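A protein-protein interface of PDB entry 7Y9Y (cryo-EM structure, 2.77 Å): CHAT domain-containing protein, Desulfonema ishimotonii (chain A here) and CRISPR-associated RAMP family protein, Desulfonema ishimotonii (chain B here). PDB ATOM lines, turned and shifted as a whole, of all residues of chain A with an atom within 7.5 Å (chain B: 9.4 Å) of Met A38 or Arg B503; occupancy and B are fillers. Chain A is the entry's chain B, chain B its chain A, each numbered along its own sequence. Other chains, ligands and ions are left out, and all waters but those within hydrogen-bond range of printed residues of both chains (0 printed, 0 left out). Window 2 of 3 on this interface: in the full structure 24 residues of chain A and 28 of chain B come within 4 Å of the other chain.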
ATOM      1  N   LYS A  32      -8.555  32.156   7.757  1.00  0.00           N
ATOM      2  CA  LYS A  32      -9.570  31.217   7.293  1.00  0.00           C
ATOM      3  C   LYS A  32      -9.660  30.008   8.216  1.00  0.00           C
ATOM      4  O   LYS A  32     -10.762  29.554   8.549  1.00  0.00           O
ATOM      5  CB  LYS A  32      -9.271  30.785   5.859  1.00  0.00           C
ATOM      6  CG  LYS A  32     -10.515  30.478   5.036  1.00  0.00           C
ATOM      7  CD  LYS A  32     -10.187  29.652   3.802  1.00  0.00           C
ATOM      8  CE  LYS A  32      -9.452  28.374   4.167  1.00  0.00           C
ATOM      9  NZ  LYS A  32      -9.483  27.385   3.055  1.00  0.00           N
ATOM     10  N   TYR A  33      -8.512  29.481   8.653  1.00  0.00           N
ATOM     11  CA  TYR A  33      -8.535  28.379   9.612  1.00  0.00           C
ATOM     12  C   TYR A  33      -9.168  28.808  10.931  1.00  0.00           C
ATOM     13  O   TYR A  33      -9.924  28.044  11.546  1.00  0.00           O
ATOM     14  CB  TYR A  33      -7.124  27.845   9.855  1.00  0.00           C
ATOM     15  CG  TYR A  33      -7.103  26.659  10.791  1.00  0.00           C
ATOM     16  CD1 TYR A  33      -7.867  25.530  10.529  1.00  0.00           C
ATOM     17  CD2 TYR A  33      -6.341  26.679  11.950  1.00  0.00           C
ATOM     18  CE1 TYR A  33      -7.860  24.449  11.387  1.00  0.00           C
ATOM     19  CE2 TYR A  33      -6.326  25.603  12.814  1.00  0.00           C
ATOM     20  CZ  TYR A  33      -7.089  24.489  12.527  1.00  0.00           C
ATOM     21  OH  TYR A  33      -7.083  23.410  13.384  1.00  0.00           O
ATOM     22  N   GLU A  34      -8.858  30.024  11.386  1.00  0.00           N
ATOM     23  CA  GLU A  34      -9.454  30.532  12.617  1.00  0.00           C
ATOM     24  C   GLU A  34     -10.971  30.605  12.468  1.00  0.00           C
ATOM     25  O   GLU A  34     -11.714  30.181  13.358  1.00  0.00           O
ATOM     26  CB  GLU A  34      -8.858  31.911  12.930  1.00  0.00           C
ATOM     27  CG  GLU A  34      -9.410  32.776  14.097  1.00  0.00           C
ATOM     28  CD  GLU A  34      -9.803  32.022  15.367  1.00  0.00           C
ATOM     29  OE1 GLU A  34      -9.187  32.310  16.410  1.00  0.00           O
ATOM     30  OE2 GLU A  34     -10.725  31.190  15.372  1.00  0.00           O
ATOM     31  N   LYS A  35     -11.445  31.082  11.316  1.00  0.00           N
ATOM     32  CA  LYS A  35     -12.882  31.159  11.069  1.00  0.00           C
ATOM     33  C   LYS A  35     -13.519  29.776  11.062  1.00  0.00           C
ATOM     34  O   LYS A  35     -14.623  29.592  11.590  1.00  0.00           O
ATOM     35  CB  LYS A  35     -13.146  31.875   9.743  1.00  0.00           C
ATOM     36  CG  LYS A  35     -14.551  32.435   9.595  1.00  0.00           C
ATOM     37  CD  LYS A  35     -14.861  33.449  10.680  1.00  0.00           C
ATOM     38  CE  LYS A  35     -15.284  34.782  10.084  1.00  0.00           C
ATOM     39  NZ  LYS A  35     -14.896  35.932  10.945  1.00  0.00           N
ATOM     40  N   GLN A  36     -12.850  28.791  10.457  1.00  0.00           N
ATOM     41  CA  GLN A  36     -13.382  27.429  10.479  1.00  0.00           C
ATOM     42  C   GLN A  36     -13.463  26.889  11.902  1.00  0.00           C
ATOM     43  O   GLN A  36     -14.413  26.179  12.248  1.00  0.00           O
ATOM     44  CB  GLN A  36     -12.540  26.498   9.604  1.00  0.00           C
ATOM     45  CG  GLN A  36     -12.302  26.989   8.190  1.00  0.00           C
ATOM     46  CD  GLN A  36     -13.156  26.262   7.170  1.00  0.00           C
ATOM     47  OE1 GLN A  36     -14.372  26.150   7.324  1.00  0.00           O
ATOM     48  NE2 GLN A  36     -12.517  25.753   6.123  1.00  0.00           N
ATOM     49  N   LEU A  37     -12.466  27.195  12.736  1.00  0.00           N
ATOM     50  CA  LEU A  37     -12.529  26.769  14.133  1.00  0.00           C
ATOM     51  C   LEU A  37     -13.664  27.460  14.882  1.00  0.00           C
ATOM     52  O   LEU A  37     -14.347  26.832  15.698  1.00  0.00           O
ATOM     53  CB  LEU A  37     -11.199  27.032  14.839  1.00  0.00           C
ATOM     54  CG  LEU A  37     -10.008  26.186  14.402  1.00  0.00           C
ATOM     55  CD1 LEU A  37      -8.782  26.551  15.222  1.00  0.00           C
ATOM     56  CD2 LEU A  37     -10.332  24.709  14.541  1.00  0.00           C
ATOM     57  N   MET A  38     -13.864  28.756  14.630  1.00  0.00           N
ATOM     58  CA  MET A  38     -14.875  29.516  15.361  1.00  0.00           C
ATOM     59  C   MET A  38     -16.273  28.984  15.078  1.00  0.00           C
ATOM     60  O   MET A  38     -17.038  28.688  16.004  1.00  0.00           O
ATOM     61  CB  MET A  38     -14.778  30.996  14.991  1.00  0.00           C
ATOM     62  CG  MET A  38     -14.933  31.944  16.162  1.00  0.00           C
ATOM     63  SD  MET A  38     -13.576  31.813  17.340  1.00  0.00           S
ATOM     64  CE  MET A  38     -14.111  32.974  18.592  1.00  0.00           C
ATOM     65  N   ASP A  39     -16.625  28.855  13.802  1.00  0.00           N
ATOM     66  CA  ASP A  39     -17.925  28.334  13.396  1.00  0.00           C
ATOM     67  C   ASP A  39     -17.813  26.820  13.260  1.00  0.00           C
ATOM     68  O   ASP A  39     -17.088  26.322  12.395  1.00  0.00           O
ATOM     69  CB  ASP A  39     -18.375  28.977  12.088  1.00  0.00           C
ATOM     70  CG  ASP A  39     -19.430  28.160  11.366  1.00  0.00           C
ATOM     71  OD1 ASP A  39     -20.388  27.700  12.022  1.00  0.00           O
ATOM     72  OD2 ASP A  39     -19.299  27.977  10.137  1.00  0.00           O
ATOM     73  N   SER A  40     -18.527  26.092  14.116  1.00  0.00           N
ATOM     74  CA  SER A  40     -18.493  24.635  14.092  1.00  0.00           C
ATOM     75  C   SER A  40     -18.884  24.112  12.718  1.00  0.00           C
ATOM     76  O   SER A  40     -19.949  24.450  12.192  1.00  0.00           O
ATOM     77  CB  SER A  40     -19.434  24.075  15.160  1.00  0.00           C
ATOM     78  OG  SER A  40     -19.011  24.444  16.460  1.00  0.00           O
ATOM     79  N   SER A  41     -18.020  23.281  12.139  1.00  0.00           N
ATOM     80  CA  SER A  41     -18.222  22.781  10.789  1.00  0.00           C
ATOM     81  C   SER A  41     -17.502  21.447  10.644  1.00  0.00           C
ATOM     82  O   SER A  41     -16.959  20.902  11.608  1.00  0.00           O
ATOM     83  CB  SER A  41     -17.727  23.793   9.752  1.00  0.00           C
ATOM     84  OG  SER A  41     -16.383  24.163  10.007  1.00  0.00           O
ATOM     85  N   THR A  44     -13.649  21.425  11.335  1.00  0.00           N
ATOM     86  CA  THR A  44     -13.145  21.228  12.687  1.00  0.00           C
ATOM     87  C   THR A  44     -12.729  19.789  12.946  1.00  0.00           C
ATOM     88  O   THR A  44     -12.065  19.527  13.955  1.00  0.00           O
ATOM     89  CB  THR A  44     -14.193  21.656  13.714  1.00  0.00           C
ATOM     90  OG1 THR A  44     -15.312  20.762  13.663  1.00  0.00           O
ATOM     91  CG2 THR A  44     -14.660  23.073  13.434  1.00  0.00           C
ATOM     92  N   HIS B 500     -22.194  28.280  34.507  1.00  0.00           N
ATOM     93  CA  HIS B 500     -21.343  28.126  33.337  1.00  0.00           C
ATOM     94  C   HIS B 500     -22.145  27.509  32.206  1.00  0.00           C
ATOM     95  O   HIS B 500     -22.925  26.579  32.420  1.00  0.00           O
ATOM     96  CB  HIS B 500     -20.143  27.235  33.647  1.00  0.00           C
ATOM     97  CG  HIS B 500     -19.206  27.814  34.656  1.00  0.00           C
ATOM     98  ND1 HIS B 500     -18.532  28.999  34.452  1.00  0.00           N
ATOM     99  CD2 HIS B 500     -18.832  27.371  35.878  1.00  0.00           C
ATOM    100  CE1 HIS B 500     -17.783  29.260  35.508  1.00  0.00           C
ATOM    101  NE2 HIS B 500     -17.947  28.288  36.386  1.00  0.00           N
ATOM    102  N   ARG B 501     -21.955  28.034  31.002  1.00  0.00           N
ATOM    103  CA  ARG B 501     -22.626  27.494  29.835  1.00  0.00           C
ATOM    104  C   ARG B 501     -21.627  27.382  28.697  1.00  0.00           C
ATOM    105  O   ARG B 501     -20.704  28.193  28.577  1.00  0.00           O
ATOM    106  CB  ARG B 501     -23.821  28.361  29.428  1.00  0.00           C
ATOM    107  CG  ARG B 501     -24.909  28.459  30.483  1.00  0.00           C
ATOM    108  CD  ARG B 501     -26.027  29.382  30.045  1.00  0.00           C
ATOM    109  NE  ARG B 501     -26.584  28.988  28.756  1.00  0.00           N
ATOM    110  CZ  ARG B 501     -27.444  29.716  28.059  1.00  0.00           C
ATOM    111  NH1 ARG B 501     -27.870  30.890  28.494  1.00  0.00           N
ATOM    112  NH2 ARG B 501     -27.889  29.254  26.894  1.00  0.00           N
ATOM    113  N   THR B 502     -21.812  26.356  27.870  1.00  0.00           N
ATOM    114  CA  THR B 502     -20.941  26.085  26.738  1.00  0.00           C
ATOM    115  C   THR B 502     -21.788  25.654  25.552  1.00  0.00           C
ATOM    116  O   THR B 502     -22.998  25.449  25.664  1.00  0.00           O
ATOM    117  CB  THR B 502     -19.903  24.999  27.055  1.00  0.00           C
ATOM    118  OG1 THR B 502     -20.562  23.840  27.581  1.00  0.00           O
ATOM    119  CG2 THR B 502     -18.890  25.497  28.059  1.00  0.00           C
ATOM    120  N   ARG B 503     -21.134  25.519  24.404  1.00  0.00           N
ATOM    121  CA  ARG B 503     -21.749  24.983  23.200  1.00  0.00           C
ATOM    122  C   ARG B 503     -20.840  23.902  22.637  1.00  0.00           C
ATOM    123  O   ARG B 503     -19.618  24.067  22.597  1.00  0.00           O
ATOM    124  CB  ARG B 503     -21.993  26.084  22.163  1.00  0.00           C
ATOM    125  CG  ARG B 503     -22.382  25.581  20.791  1.00  0.00           C
ATOM    126  CD  ARG B 503     -22.922  26.701  19.929  1.00  0.00           C
ATOM    127  NE  ARG B 503     -21.923  27.180  18.982  1.00  0.00           N
ATOM    128  CZ  ARG B 503     -21.096  28.191  19.210  1.00  0.00           C
ATOM    129  NH1 ARG B 503     -21.137  28.876  20.341  1.00  0.00           N
ATOM    130  NH2 ARG B 503     -20.206  28.522  18.280  1.00  0.00           N
ATOM    131  N   ILE B 504     -21.440  22.797  22.207  1.00  0.00           N
ATOM    132  CA  ILE B 504     -20.711  21.610  21.776  1.00  0.00           C
ATOM    133  C   ILE B 504     -20.678  21.573  20.256  1.00  0.00           C
ATOM    134  O   ILE B 504     -21.700  21.808  19.599  1.00  0.00           O
ATOM    135  CB  ILE B 504     -21.351  20.332  22.344  1.00  0.00           C
ATOM    136  CG1 ILE B 504     -21.380  20.381  23.871  1.00  0.00           C
ATOM    137  CG2 ILE B 504     -20.613  19.099  21.862  1.00  0.00           C
ATOM    138  CD1 ILE B 504     -20.022  20.311  24.511  1.00  0.00           C
ATOM    139  N   ASN B 505     -19.507  21.291  19.698  1.00  0.00           N
ATOM    140  CA  ASN B 505     -19.380  21.074  18.261  1.00  0.00           C
ATOM    141  C   ASN B 505     -19.978  19.718  17.909  1.00  0.00           C
ATOM    142  O   ASN B 505     -19.520  18.696  18.437  1.00  0.00           O
ATOM    143  CB  ASN B 505     -17.912  21.148  17.844  1.00  0.00           C
ATOM    144  CG  ASN B 505     -17.700  20.837  16.374  1.00  0.00           C
ATOM    145  OD1 ASN B 505     -18.629  20.886  15.573  1.00  0.00           O
ATOM    146  ND2 ASN B 505     -16.463  20.528  16.009  1.00  0.00           N
ATOM    147  N   PRO B 506     -20.997  19.657  17.048  1.00  0.00           N
ATOM    148  CA  PRO B 506     -21.638  18.362  16.764  1.00  0.00           C
ATOM    149  C   PRO B 506     -20.708  17.327  16.158  1.00  0.00           C
ATOM    150  O   PRO B 506     -20.878  16.131  16.424  1.00  0.00           O
ATOM    151  CB  PRO B 506     -22.771  18.738  15.798  1.00  0.00           C
ATOM    152  CG  PRO B 506     -22.418  20.090  15.280  1.00  0.00           C
ATOM    153  CD  PRO B 506     -21.694  20.771  16.389  1.00  0.00           C
ATOM    154  N   THR B 508     -17.048  16.918  16.259  1.00  0.00           N
ATOM    155  CA  THR B 508     -16.020  16.350  17.125  1.00  0.00           C
ATOM    156  C   THR B 508     -16.600  15.835  18.436  1.00  0.00           C
ATOM    157  O   THR B 508     -16.087  14.864  19.002  1.00  0.00           O
ATOM    158  CB  THR B 508     -14.928  17.383  17.404  1.00  0.00           C
ATOM    159  OG1 THR B 508     -15.466  18.455  18.183  1.00  0.00           O
ATOM    160  CG2 THR B 508     -14.385  17.934  16.105  1.00  0.00           C
ATOM    161  N   GLY B 509     -17.664  16.464  18.930  1.00  0.00           N
ATOM    162  CA  GLY B 509     -18.253  16.096  20.199  1.00  0.00           C
ATOM    163  C   GLY B 509     -17.727  16.858  21.394  1.00  0.00           C
ATOM    164  O   GLY B 509     -18.182  16.606  22.517  1.00  0.00           O
ATOM    165  N   THR B 510     -16.787  17.775  21.194  1.00  0.00           N
ATOM    166  CA  THR B 510     -16.253  18.621  22.249  1.00  0.00           C
ATOM    167  C   THR B 510     -16.726  20.054  22.045  1.00  0.00           C
ATOM    168  O   THR B 510     -17.431  20.369  21.085  1.00  0.00           O
ATOM    169  CB  THR B 510     -14.721  18.553  22.288  1.00  0.00           C
ATOM    170  OG1 THR B 510     -14.172  19.527  21.395  1.00  0.00           O
ATOM    171  CG2 THR B 510     -14.235  17.174  21.886  1.00  0.00           C
ATOM    172  N   VAL B 511     -16.328  20.927  22.971  1.00  0.00           N
ATOM    173  CA  VAL B 511     -16.813  22.301  22.960  1.00  0.00           C
ATOM    174  C   VAL B 511     -16.285  23.040  21.736  1.00  0.00           C
ATOM    175  O   VAL B 511     -15.232  22.704  21.180  1.00  0.00           O
ATOM    176  CB  VAL B 511     -16.415  23.033  24.254  1.00  0.00           C
ATOM    177  CG1 VAL B 511     -17.199  22.495  25.431  1.00  0.00           C
ATOM    178  CG2 VAL B 511     -14.921  22.909  24.495  1.00  0.00           C
ATOM    179  N   ALA B 512     -17.028  24.058  21.316  1.00  0.00           N
ATOM    180  CA  ALA B 512     -16.618  24.902  20.206  1.00  0.00           C
ATOM    181  C   ALA B 512     -15.631  25.964  20.677  1.00  0.00           C
ATOM    182  O   ALA B 512     -15.413  26.153  21.877  1.00  0.00           O
ATOM    183  CB  ALA B 512     -17.832  25.565  19.559  1.00  0.00           C
ATOM    184  N   GLU B 513     -15.022  26.653  19.715  1.00  0.00           N
ATOM    185  CA  GLU B 513     -14.043  27.678  20.042  1.00  0.00           C
ATOM    186  C   GLU B 513     -14.732  28.921  20.589  1.00  0.00           C
ATOM    187  O   GLU B 513     -15.596  29.508  19.935  1.00  0.00           O
ATOM    188  CB  GLU B 513     -13.219  28.034  18.805  1.00  0.00           C
ATOM    189  CG  GLU B 513     -11.864  27.355  18.747  1.00  0.00           C
ATOM    190  CD  GLU B 513     -10.834  28.033  19.625  1.00  0.00           C
ATOM    191  OE1 GLU B 513     -10.074  27.316  20.309  1.00  0.00           O
ATOM    192  OE2 GLU B 513     -10.788  29.282  19.637  1.00  0.00           O
ATOM    193  N   GLY B 514     -14.344  29.319  21.798  1.00  0.00           N
ATOM    194  CA  GLY B 514     -14.887  30.498  22.431  1.00  0.00           C
ATOM    195  C   GLY B 514     -16.226  30.304  23.105  1.00  0.00           C
ATOM    196  O   GLY B 514     -16.725  31.245  23.734  1.00  0.00           O
ATOM    197  N   ALA B 515     -16.819  29.115  23.003  1.00  0.00           N
ATOM    198  CA  ALA B 515     -18.151  28.856  23.550  1.00  0.00           C
ATOM    199  C   ALA B 515     -18.038  28.464  25.024  1.00  0.00           C
ATOM    200  O   ALA B 515     -18.169  27.304  25.413  1.00  0.00           O
ATOM    201  CB  ALA B 515     -18.856  27.782  22.736  1.00  0.00           C
ATOM    202  N   LEU B 516     -17.784  29.475  25.850  1.00  0.00           N
ATOM    203  CA  LEU B 516     -17.734  29.301  27.297  1.00  0.00           C
ATOM    204  C   LEU B 516     -18.072  30.635  27.939  1.00  0.00           C
ATOM    205  O   LEU B 516     -17.320  31.602  27.783  1.00  0.00           O
ATOM    206  CB  LEU B 516     -16.357  28.808  27.751  1.00  0.00           C
ATOM    207  CG  LEU B 516     -16.072  28.769  29.255  1.00  0.00           C
ATOM    208  CD1 LEU B 516     -17.093  27.925  29.995  1.00  0.00           C
ATOM    209  CD2 LEU B 516     -14.668  28.258  29.514  1.00  0.00           C
ATOM    210  N   PHE B 517     -19.196  30.694  28.651  1.00  0.00           N
ATOM    211  CA  PHE B 517     -19.656  31.958  29.203  1.00  0.00           C
ATOM    212  C   PHE B 517     -20.313  31.747  30.559  1.00  0.00           C
ATOM    213  O   PHE B 517     -20.609  30.622  30.970  1.00  0.00           O
ATOM    214  CB  PHE B 517     -20.624  32.693  28.260  1.00  0.00           C
ATOM    215  CG  PHE B 517     -21.717  31.833  27.684  1.00  0.00           C
ATOM    216  CD1 PHE B 517     -21.444  30.880  26.714  1.00  0.00           C
ATOM    217  CD2 PHE B 517     -23.027  32.004  28.091  1.00  0.00           C
ATOM    218  CE1 PHE B 517     -22.450  30.103  26.185  1.00  0.00           C
ATOM    219  CE2 PHE B 517     -24.035  31.234  27.561  1.00  0.00           C
ATOM    220  CZ  PHE B 517     -23.746  30.281  26.609  1.00  0.00           C
ATOM    221  N   GLU B 677     -30.048  24.048  30.767  1.00  0.00           N
ATOM    222  CA  GLU B 677     -29.302  24.195  29.522  1.00  0.00           C
ATOM    223  C   GLU B 677     -28.731  22.866  29.049  1.00  0.00           C
ATOM    224  O   GLU B 677     -28.768  22.567  27.852  1.00  0.00           O
ATOM    225  CB  GLU B 677     -28.183  25.219  29.703  1.00  0.00           C
ATOM    226  CG  GLU B 677     -28.642  26.560  30.253  1.00  0.00           C
ATOM    227  CD  GLU B 677     -28.732  26.587  31.765  1.00  0.00           C
ATOM    228  OE1 GLU B 677     -28.233  25.645  32.409  1.00  0.00           O
ATOM    229  OE2 GLU B 677     -29.306  27.551  32.312  1.00  0.00           O
ATOM    230  N   GLY B 681     -29.737  20.978  25.621  1.00  0.00           N
ATOM    231  CA  GLY B 681     -28.747  20.641  24.612  1.00  0.00           C
ATOM    232  C   GLY B 681     -28.747  19.170  24.251  1.00  0.00           C
ATOM    233  O   GLY B 681     -28.657  18.812  23.074  1.00  0.00           O
ATOM    234  N   ARG B 684     -31.884  18.496  22.191  1.00  0.00           N
ATOM    235  CA  ARG B 684     -31.739  19.081  20.864  1.00  0.00           C
ATOM    236  C   ARG B 684     -30.807  18.250  19.993  1.00  0.00           C
ATOM    237  O   ARG B 684     -31.064  18.061  18.799  1.00  0.00           O
ATOM    238  CB  ARG B 684     -31.236  20.519  20.993  1.00  0.00           C
ATOM    239  CG  ARG B 684     -30.848  21.174  19.689  1.00  0.00           C
ATOM    240  CD  ARG B 684     -30.619  22.666  19.874  1.00  0.00           C
ATOM    241  NE  ARG B 684     -30.868  23.445  18.665  1.00  0.00           N
ATOM    242  CZ  ARG B 684     -30.317  23.228  17.476  1.00  0.00           C
ATOM    243  NH1 ARG B 684     -29.375  22.315  17.302  1.00  0.00           N
ATOM    244  NH2 ARG B 684     -30.706  23.961  16.438  1.00  0.00           N
ATOM    245  N   PRO B1329      -4.013  30.592  17.796  1.00  0.00           N
ATOM    246  CA  PRO B1329      -4.597  29.240  17.789  1.00  0.00           C
ATOM    247  C   PRO B1329      -3.740  28.191  17.101  1.00  0.00           C
ATOM    248  O   PRO B1329      -3.718  27.037  17.552  1.00  0.00           O
ATOM    249  CB  PRO B1329      -5.930  29.448  17.057  1.00  0.00           C
ATOM    250  CG  PRO B1329      -5.675  30.602  16.151  1.00  0.00           C
ATOM    251  CD  PRO B1329      -4.699  31.503  16.864  1.00  0.00           C
ATOM    252  N   ARG B1332      -1.939  24.844  18.390  1.00  0.00           N
ATOM    253  CA  ARG B1332      -2.441  23.480  18.519  1.00  0.00           C
ATOM    254  C   ARG B1332      -1.933  22.599  17.384  1.00  0.00           C
ATOM    255  O   ARG B1332      -1.785  21.382  17.549  1.00  0.00           O
ATOM    256  CB  ARG B1332      -3.971  23.476  18.568  1.00  0.00           C
ATOM    257  CG  ARG B1332      -4.649  23.394  17.211  1.00  0.00           C
ATOM    258  CD  ARG B1332      -6.127  23.706  17.311  1.00  0.00           C
ATOM    259  NE  ARG B1332      -6.375  25.002  17.928  1.00  0.00           N
ATOM    260  CZ  ARG B1332      -7.450  25.291  18.647  1.00  0.00           C
ATOM    261  NH1 ARG B1332      -8.401  24.397  18.858  1.00  0.00           N
ATOM    262  NH2 ARG B1332      -7.574  26.509  19.168  1.00  0.00           N
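Of the 11 printed residues of chain A, 5 touch a printed residue of chain B. Hydrophobic or aromatic side chains of chain A within 4 Å of the printed part of chain B: Leu A37. Of the 22 printed residues of chain B, 7 touch a printed residue of chain A. Among the printed residues, no Asp or Glu carboxylate lies within 4 Å of a Lys or Arg side-chain nitrogen of the other chain.
O of Arg B503 is in hydrogen-bond range of N of Ala B512 (2.9 Å). ND2 of Asn B505 sits at hydrogen-bond distance from OG1 of Thr B508 (3.2 Å). The backbone NH (N) of Asn B505 is in hydrogen-bond range of the backbone carbonyl oxygen (O) of Thr B510. The backbone NH (N) of Thr B510 sits at hydrogen-bond distance from the side-chain hydroxyl (OG1) of Thr B508, 3.4 Å away. The backbone carbonyl oxygen (O) of Pro B1329 lies within hydrogen-bond range of the guanidinium group (NE) of Arg B1332 (3.4 Å). The backbone carbonyl oxygen of Ser A41 is in hydrogen-bond range of the side-chain hydroxyl of Thr A44 (2.6 Å).
Among the printed residues, pairs that only touch across the chains: Ser A40 with Asn B505 (3.3 Å), Ser A40 with Ala B512 (3.5 Å), Leu A37 with Glu B513 (3.5 Å), Thr A44 with Thr B508 (3.5 Å), Leu A37 with Arg B1332 (3.9 Å), Met A38 with Arg B503 (3.9 Å) and Glu A34 with Pro B1329 (3.9 Å).
The side-chain hydroxyl (OG1) of Thr A44 sits at hydrogen-bond distance from the side-chain amide nitrogen (ND2) of Asn B505 (2.6 Å).
Printed residues of chain B within 4 Å of Met A38: Arg B503. Arg B503 touches just one residue of chain A: Met A38. Of the printed residues of chain B, Glu A34 touches Pro B1329. Of the printed residues of chain A, Thr B508 touches Thr A44. Of the printed residues of chain B, Ser A40 touches Asn B505 and Ala B512. Of the printed residues of chain A, Arg B1332 touches Leu A37 (3.9 Å). Printed residues of chain A within 4 Å of Pro B1329: Glu A34. Gly B514 touches none of the printed residues of chain A. The nearest printed residue of chain B that does not touch Met A38 is Glu B513 (4.003 Å). The nearest residue of chain A that does not touch Arg B503 is Ser A40 (4.6 Å).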
